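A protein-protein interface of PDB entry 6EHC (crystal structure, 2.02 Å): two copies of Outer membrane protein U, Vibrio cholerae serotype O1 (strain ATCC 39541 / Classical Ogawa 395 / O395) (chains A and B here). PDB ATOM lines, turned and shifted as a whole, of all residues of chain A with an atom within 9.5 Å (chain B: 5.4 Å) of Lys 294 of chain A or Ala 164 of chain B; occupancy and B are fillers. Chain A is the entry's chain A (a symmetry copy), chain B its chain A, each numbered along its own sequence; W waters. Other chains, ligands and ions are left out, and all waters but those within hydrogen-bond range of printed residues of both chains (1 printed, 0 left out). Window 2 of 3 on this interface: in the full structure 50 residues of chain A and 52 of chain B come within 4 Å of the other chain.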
ATOM      1  N   LYS A  24     -23.758 -20.415 -32.689  1.00  0.00           N
ATOM      2  CA  LYS A  24     -23.431 -21.579 -31.846  1.00  0.00           C
ATOM      3  C   LYS A  24     -24.689 -22.443 -31.714  1.00  0.00           C
ATOM      4  O   LYS A  24     -25.720 -21.946 -31.211  1.00  0.00           O
ATOM      5  CB  LYS A  24     -22.970 -21.166 -30.432  1.00  0.00           C
ATOM      6  CG  LYS A  24     -21.616 -20.434 -30.388  1.00  0.00           C
ATOM      7  CD  LYS A  24     -21.160 -20.238 -28.963  1.00  0.00           C
ATOM      8  CE  LYS A  24     -20.044 -19.234 -28.845  1.00  0.00           C
ATOM      9  NZ  LYS A  24     -19.378 -19.340 -27.506  1.00  0.00           N
ATOM     10  N   ASP A  25     -24.627 -23.704 -32.192  1.00  0.00           N
ATOM     11  CA  ASP A  25     -25.780 -24.662 -32.180  1.00  0.00           C
ATOM     12  C   ASP A  25     -26.987 -24.063 -32.900  1.00  0.00           C
ATOM     13  O   ASP A  25     -28.114 -24.138 -32.429  1.00  0.00           O
ATOM     14  CB  ASP A  25     -26.117 -25.030 -30.725  1.00  0.00           C
ATOM     15  CG  ASP A  25     -27.134 -26.183 -30.581  1.00  0.00           C
ATOM     16  OD1 ASP A  25     -27.273 -27.030 -31.483  1.00  0.00           O
ATOM     17  OD2 ASP A  25     -27.783 -26.229 -29.510  1.00  0.00           O
ATOM     18  N   LYS A  27     -27.857 -20.926 -33.171  1.00  0.00           N
ATOM     19  CA  LYS A  27     -28.514 -19.790 -32.491  1.00  0.00           C
ATOM     20  C   LYS A  27     -27.597 -18.559 -32.510  1.00  0.00           C
ATOM     21  O   LYS A  27     -26.351 -18.663 -32.178  1.00  0.00           O
ATOM     22  CB  LYS A  27     -28.839 -20.186 -31.069  1.00  0.00           C
ATOM     23  CG  LYS A  27     -29.888 -21.319 -30.999  1.00  0.00           C
ATOM     24  CD  LYS A  27     -29.600 -22.221 -29.814  1.00  0.00           C
ATOM     25  CE  LYS A  27     -30.628 -23.350 -29.714  1.00  0.00           C
ATOM     26  NZ  LYS A  27     -30.417 -24.296 -30.826  1.00  0.00           N
ATOM     27  N   ASN A 285     -14.037 -26.487 -31.249  1.00  0.00           N
ATOM     28  CA  ASN A 285     -13.747 -26.561 -29.831  1.00  0.00           C
ATOM     29  C   ASN A 285     -13.667 -28.033 -29.484  1.00  0.00           C
ATOM     30  O   ASN A 285     -14.681 -28.724 -29.488  1.00  0.00           O
ATOM     31  CB  ASN A 285     -14.866 -25.909 -29.039  1.00  0.00           C
ATOM     32  CG  ASN A 285     -14.597 -25.844 -27.559  1.00  0.00           C
ATOM     33  OD1 ASN A 285     -13.796 -26.578 -27.001  1.00  0.00           O
ATOM     34  ND2 ASN A 285     -15.305 -24.962 -26.904  1.00  0.00           N
ATOM     35  N   LEU A 286     -12.462 -28.472 -29.116  1.00  0.00           N
ATOM     36  CA  LEU A 286     -12.119 -29.910 -28.969  1.00  0.00           C
ATOM     37  C   LEU A 286     -12.086 -30.402 -27.523  1.00  0.00           C
ATOM     38  O   LEU A 286     -11.729 -31.550 -27.303  1.00  0.00           O
ATOM     39  CB  LEU A 286     -10.748 -30.196 -29.625  1.00  0.00           C
ATOM     40  CG  LEU A 286     -10.535 -29.560 -30.991  1.00  0.00           C
ATOM     41  CD1 LEU A 286      -9.084 -29.651 -31.398  1.00  0.00           C
ATOM     42  CD2 LEU A 286     -11.452 -30.204 -32.022  1.00  0.00           C
ATOM     43  N   LEU A 287     -12.469 -29.583 -26.538  1.00  0.00           N
ATOM     44  CA  LEU A 287     -12.699 -30.126 -25.181  1.00  0.00           C
ATOM     45  C   LEU A 287     -13.779 -31.226 -25.230  1.00  0.00           C
ATOM     46  O   LEU A 287     -14.769 -31.072 -25.949  1.00  0.00           O
ATOM     47  CB  LEU A 287     -13.162 -29.032 -24.221  1.00  0.00           C
ATOM     48  CG  LEU A 287     -12.283 -27.798 -23.963  1.00  0.00           C
ATOM     49  CD1 LEU A 287     -13.066 -26.739 -23.213  1.00  0.00           C
ATOM     50  CD2 LEU A 287     -11.030 -28.154 -23.208  1.00  0.00           C
ATOM     51  N   ASP A 288     -13.604 -32.320 -24.485  1.00  0.00           N
ATOM     52  CA  ASP A 288     -14.667 -33.371 -24.354  1.00  0.00           C
ATOM     53  C   ASP A 288     -15.571 -33.148 -23.140  1.00  0.00           C
ATOM     54  O   ASP A 288     -15.353 -32.214 -22.372  1.00  0.00           O
ATOM     55  CB  ASP A 288     -14.057 -34.788 -24.285  1.00  0.00           C
ATOM     56  CG  ASP A 288     -13.344 -35.089 -22.942  1.00  0.00           C
ATOM     57  OD1 ASP A 288     -14.013 -35.334 -21.904  1.00  0.00           O
ATOM     58  OD2 ASP A 288     -12.095 -35.118 -22.943  1.00  0.00           O
ATOM     59  N   SER A 289     -16.569 -34.024 -22.974  1.00  0.00           N
ATOM     60  CA  SER A 289     -17.327 -34.172 -21.715  1.00  0.00           C
ATOM     61  C   SER A 289     -16.935 -35.463 -20.977  1.00  0.00           C
ATOM     62  O   SER A 289     -16.390 -35.419 -19.866  1.00  0.00           O
ATOM     63  CB  SER A 289     -18.824 -34.174 -21.994  1.00  0.00           C
ATOM     64  OG  SER A 289     -19.140 -35.193 -22.917  1.00  0.00           O
ATOM     65  N   ALA A 292     -15.699 -30.905 -19.370  1.00  0.00           N
ATOM     66  CA  ALA A 292     -16.352 -29.706 -19.902  1.00  0.00           C
ATOM     67  C   ALA A 292     -17.842 -29.897 -20.170  1.00  0.00           C
ATOM     68  O   ALA A 292     -18.248 -30.946 -20.673  1.00  0.00           O
ATOM     69  CB  ALA A 292     -15.666 -29.260 -21.179  1.00  0.00           C
ATOM     70  N   SER A 293     -18.648 -28.875 -19.866  1.00  0.00           N
ATOM     71  CA  SER A 293     -20.080 -28.925 -20.165  1.00  0.00           C
ATOM     72  C   SER A 293     -20.294 -28.787 -21.674  1.00  0.00           C
ATOM     73  O   SER A 293     -19.340 -28.506 -22.441  1.00  0.00           O
ATOM     74  CB  SER A 293     -20.862 -27.856 -19.392  1.00  0.00           C
ATOM     75  OG  SER A 293     -20.854 -26.599 -20.058  1.00  0.00           O
ATOM     76  N   LYS A 294     -21.544 -28.979 -22.101  1.00  0.00           N
ATOM     77  CA  LYS A 294     -21.898 -28.830 -23.508  1.00  0.00           C
ATOM     78  C   LYS A 294     -21.590 -27.415 -24.021  1.00  0.00           C
ATOM     79  O   LYS A 294     -20.870 -27.268 -25.020  1.00  0.00           O
ATOM     80  CB  LYS A 294     -23.347 -29.207 -23.757  1.00  0.00           C
ATOM     81  CG  LYS A 294     -23.566 -29.731 -25.154  1.00  0.00           C
ATOM     82  CD  LYS A 294     -24.990 -30.209 -25.357  1.00  0.00           C
ATOM     83  CE  LYS A 294     -25.863 -29.116 -25.951  1.00  0.00           C
ATOM     84  NZ  LYS A 294     -27.207 -29.658 -26.314  1.00  0.00           N
ATOM     85  N   VAL A 295     -22.076 -26.402 -23.297  1.00  0.00           N
ATOM     86  CA  VAL A 295     -21.750 -24.957 -23.551  1.00  0.00           C
ATOM     87  C   VAL A 295     -20.253 -24.642 -23.735  1.00  0.00           C
ATOM     88  O   VAL A 295     -19.841 -24.050 -24.743  1.00  0.00           O
ATOM     89  CB  VAL A 295     -22.321 -24.046 -22.430  1.00  0.00           C
ATOM     90  CG1 VAL A 295     -21.657 -22.655 -22.399  1.00  0.00           C
ATOM     91  CG2 VAL A 295     -23.829 -23.914 -22.609  1.00  0.00           C
ATOM     92  N   ALA A 296     -19.465 -25.013 -22.738  1.00  0.00           N
ATOM     93  CA  ALA A 296     -18.005 -24.898 -22.797  1.00  0.00           C
ATOM     94  C   ALA A 296     -17.344 -25.576 -24.031  1.00  0.00           C
ATOM     95  O   ALA A 296     -16.265 -25.139 -24.424  1.00  0.00           O
ATOM     96  CB  ALA A 296     -17.393 -25.454 -21.511  1.00  0.00           C
ATOM     97  N   SER A 297     -18.003 -26.592 -24.628  1.00  0.00           N
ATOM     98  CA  SER A 297     -17.520 -27.377 -25.789  1.00  0.00           C
ATOM     99  C   SER A 297     -18.075 -27.025 -27.181  1.00  0.00           C
ATOM    100  O   SER A 297     -17.625 -27.630 -28.147  1.00  0.00           O
ATOM    101  CB  SER A 297     -17.840 -28.873 -25.584  1.00  0.00           C
ATOM    102  OG  SER A 297     -17.296 -29.338 -24.368  1.00  0.00           O
ATOM    103  N   GLU A 298     -19.054 -26.119 -27.300  1.00  0.00           N
ATOM    104  CA  GLU A 298     -19.666 -25.846 -28.607  1.00  0.00           C
ATOM    105  C   GLU A 298     -18.764 -25.125 -29.588  1.00  0.00           C
ATOM    106  O   GLU A 298     -18.091 -24.147 -29.228  1.00  0.00           O
ATOM    107  CB  GLU A 298     -20.919 -24.993 -28.487  1.00  0.00           C
ATOM    108  CG  GLU A 298     -22.063 -25.700 -27.811  1.00  0.00           C
ATOM    109  CD  GLU A 298     -22.902 -26.562 -28.725  1.00  0.00           C
ATOM    110  OE1 GLU A 298     -22.598 -26.669 -29.947  1.00  0.00           O
ATOM    111  OE2 GLU A 298     -23.889 -27.117 -28.161  1.00  0.00           O
ATOM    112  N   ASP A 299     -18.796 -25.597 -30.838  1.00  0.00           N
ATOM    113  CA  ASP A 299     -18.119 -24.941 -31.946  1.00  0.00           C
ATOM    114  C   ASP A 299     -18.744 -23.562 -32.205  1.00  0.00           C
ATOM    115  O   ASP A 299     -19.853 -23.286 -31.711  1.00  0.00           O
ATOM    116  CB  ASP A 299     -18.252 -25.783 -33.203  1.00  0.00           C
ATOM    117  CG  ASP A 299     -17.418 -27.125 -33.154  1.00  0.00           C
ATOM    118  OD1 ASP A 299     -16.787 -27.540 -32.134  1.00  0.00           O
ATOM    119  OD2 ASP A 299     -17.437 -27.754 -34.210  1.00  0.00           O
ATOM    120  N   VAL B 151     -28.972 -21.663 -20.906  1.00  0.00           N
ATOM    121  CA  VAL B 151     -29.869 -22.174 -19.868  1.00  0.00           C
ATOM    122  C   VAL B 151     -29.299 -23.376 -19.098  1.00  0.00           C
ATOM    123  O   VAL B 151     -28.457 -24.140 -19.610  1.00  0.00           O
ATOM    124  CB  VAL B 151     -31.263 -22.527 -20.424  1.00  0.00           C
ATOM    125  CG1 VAL B 151     -31.930 -21.294 -21.020  1.00  0.00           C
ATOM    126  CG2 VAL B 151     -31.197 -23.638 -21.462  1.00  0.00           C
ATOM    127  N   ASP B 152     -29.780 -23.526 -17.863  1.00  0.00           N
ATOM    128  CA  ASP B 152     -29.492 -24.695 -17.018  1.00  0.00           C
ATOM    129  C   ASP B 152     -30.207 -25.929 -17.549  1.00  0.00           C
ATOM    130  O   ASP B 152     -30.948 -25.857 -18.537  1.00  0.00           O
ATOM    131  CB  ASP B 152     -29.824 -24.412 -15.527  1.00  0.00           C
ATOM    132  CG  ASP B 152     -31.312 -24.219 -15.246  1.00  0.00           C
ATOM    133  OD1 ASP B 152     -32.175 -24.485 -16.107  1.00  0.00           O
ATOM    134  OD2 ASP B 152     -31.633 -23.791 -14.124  1.00  0.00           O
ATOM    135  N   ALA B 153     -30.012 -27.057 -16.885  1.00  0.00           N
ATOM    136  CA  ALA B 153     -30.583 -28.340 -17.332  1.00  0.00           C
ATOM    137  C   ALA B 153     -32.109 -28.404 -17.239  1.00  0.00           C
ATOM    138  O   ALA B 153     -32.737 -29.256 -17.876  1.00  0.00           O
ATOM    139  CB  ALA B 153     -29.944 -29.496 -16.568  1.00  0.00           C
ATOM    140  N   ASN B 162     -22.038 -21.315 -15.895  1.00  0.00           N
ATOM    141  CA  ASN B 162     -22.829 -22.384 -15.239  1.00  0.00           C
ATOM    142  C   ASN B 162     -23.998 -23.032 -16.059  1.00  0.00           C
ATOM    143  O   ASN B 162     -24.828 -23.774 -15.496  1.00  0.00           O
ATOM    144  CB  ASN B 162     -23.302 -21.872 -13.860  1.00  0.00           C
ATOM    145  CG  ASN B 162     -22.140 -21.436 -12.960  1.00  0.00           C
ATOM    146  OD1 ASN B 162     -21.083 -22.076 -12.910  1.00  0.00           O
ATOM    147  ND2 ASN B 162     -22.325 -20.332 -12.262  1.00  0.00           N
ATOM    148  N   ALA B 163     -24.036 -22.812 -17.375  1.00  0.00           N
ATOM    149  CA  ALA B 163     -25.149 -23.298 -18.205  1.00  0.00           C
ATOM    150  C   ALA B 163     -24.933 -24.720 -18.722  1.00  0.00           C
ATOM    151  O   ALA B 163     -23.823 -25.198 -18.810  1.00  0.00           O
ATOM    152  CB  ALA B 163     -25.400 -22.351 -19.375  1.00  0.00           C
ATOM    153  N   ALA B 164     -26.024 -25.391 -19.049  1.00  0.00           N
ATOM    154  CA  ALA B 164     -25.987 -26.734 -19.575  1.00  0.00           C
ATOM    155  C   ALA B 164     -25.866 -26.631 -21.101  1.00  0.00           C
ATOM    156  O   ALA B 164     -24.924 -27.202 -21.672  1.00  0.00           O
ATOM    157  CB  ALA B 164     -27.231 -27.502 -19.167  1.00  0.00           C
ATOM    158  N   LYS B 165     -26.755 -25.849 -21.733  1.00  0.00           N
ATOM    159  CA  LYS B 165     -26.878 -25.773 -23.207  1.00  0.00           C
ATOM    160  C   LYS B 165     -27.311 -24.391 -23.642  1.00  0.00           C
ATOM    161  O   LYS B 165     -27.767 -23.622 -22.826  1.00  0.00           O
ATOM    162  CB  LYS B 165     -27.914 -26.779 -23.705  1.00  0.00           C
ATOM    163  CG  LYS B 165     -29.324 -26.455 -23.210  1.00  0.00           C
ATOM    164  CD  LYS B 165     -30.327 -27.609 -23.266  1.00  0.00           C
ATOM    165  CE  LYS B 165     -31.241 -27.587 -22.030  1.00  0.00           C
ATOM    166  NZ  LYS B 165     -32.683 -27.590 -22.365  1.00  0.00           N
ATOM    167  N   TYR B 166     -27.191 -24.100 -24.930  1.00  0.00           N
ATOM    168  CA  TYR B 166     -27.736 -22.867 -25.490  1.00  0.00           C
ATOM    169  C   TYR B 166     -29.191 -23.047 -25.882  1.00  0.00           C
ATOM    170  O   TYR B 166     -29.561 -24.099 -26.369  1.00  0.00           O
ATOM    171  CB  TYR B 166     -26.955 -22.422 -26.728  1.00  0.00           C
ATOM    172  CG  TYR B 166     -25.598 -21.926 -26.394  1.00  0.00           C
ATOM    173  CD1 TYR B 166     -25.440 -20.763 -25.630  1.00  0.00           C
ATOM    174  CD2 TYR B 166     -24.456 -22.638 -26.754  1.00  0.00           C
ATOM    175  CE1 TYR B 166     -24.187 -20.297 -25.274  1.00  0.00           C
ATOM    176  CE2 TYR B 166     -23.190 -22.163 -26.405  1.00  0.00           C
ATOM    177  CZ  TYR B 166     -23.062 -20.983 -25.674  1.00  0.00           C
ATOM    178  OH  TYR B 166     -21.820 -20.498 -25.293  1.00  0.00           O
HETATM  179  O   HOH W   1     -25.929 -26.036 -26.808  1.00  0.00           O
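Among the printed residues, merely in contact across the chains: Lys 27 of chain A with Tyr 166 of chain B (3.6 Å), Ser 293 of chain A with Ala 163 of chain B (3.5 Å), Lys 294 of chain A with Ala 164 of chain B (3.3 Å), Lys 294 of chain A with Lys 165 of chain B (3.8 Å), Val 295 of chain A with Ala 163 of chain B (3.9 Å), Val 295 of chain A with Lys 165 of chain B (3.6 Å), Val 295 of chain A with Tyr 166 of chain B (3.6 Å) and Glu 298 of chain A with Tyr 166 of chain B (3.97 Å).
The backbone carbonyl oxygen (O) of Ala 164 of chain B lies within hydrogen-bond range of the backbone NH (N) of Val 295 of chain A (3.4 Å). The side-chain hydroxyl (OH) of Tyr 166 of chain B is in hydrogen-bond range of the side-chain amino group (NZ) of Lys 24 of chain A (3.5 Å).
Lys 294 of chain A touches two residues of chain B. Ala 163 of chain B touches just these residues of chain A: Ser 293 and Val 295. Of the printed residues of chain A, Lys 165 of chain B touches Lys 294 and Val 295. Of the printed residues of chain B, Lys 27 of chain A touches Tyr 166. Of the printed residues of chain B, Val 295 of chain A touches Ala 163, Ala 164, Lys 165 and Tyr 166. Of the printed residues of chain A, Tyr 166 of chain B touches Lys 24 (3.5 Å), Lys 27 (3.6 Å), Val 295 (3.6 Å) and Glu 298 (3.97 Å). Leu 286 of chain A touches none of the printed residues of chain B. Asp 288 of chain A touches none of the printed residues of chain B. The nearest residue of chain B that does not touch Lys 294 of chain A is Tyr 166 of chain B (5.3 Å). The nearest residue of chain A that does not touch Ala 164 of chain B is Ser 293 of chain A (4.4 Å).
Of the 16 printed residues of chain A, 6 touch a printed residue of chain B. Of the 8 printed residues of chain B, 4 touch a printed residue of chain A. Printed residues of chain B that touch a printed residue of chain A: Ala 163, Ala 164, Lys 165 and Tyr 166. Hydrophobic or aromatic side chains of chain B within 4 Å of the printed part of chain A: Ala 163 and Tyr 166. Among the printed residues, no Asp or Glu carboxylate lies within 4 Å of a Lys or Arg side-chain nitrogen of the other chain.
The backbone carbonyl oxygen (O) of Val 151 of chain B is in hydrogen-bond range of the backbone NH (N) of Ala 164 of chain B (2.8 Å). The backbone NH (N) of Val 151 of chain B sits at hydrogen-bond distance from the backbone carbonyl oxygen (O) of Lys 165 of chain B (3.0 Å). The side-chain carboxylate (OD2) of Asp 25 of chain A is in salt-bridge range of the side-chain amino group (NZ) of Lys 27 of chain A, at 3.5 Å. OG of Ser 293 of chain A lies close to N of Val 295 of chain A (3.5 Å). OG of Ser 293 of chain A sits at hydrogen-bond distance from N of Ala 296 of chain A (3.4 Å). O of Ser 293 of chain A is in hydrogen-bond range of OG of Ser 297 of chain A, 2.9 Å away.
Water W1 lies within hydrogen-bond range of OE2 of Glu 298 of chain A (2.7 Å), N of Tyr 166 of chain B (3.0 Å) and OD2 of Asp 25 of chain A (3.3 Å).
No position is printed for both chains. Of the 10 pairs that touch across the chains among the printed residues, none has its exchanged pair printed and touching as well.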
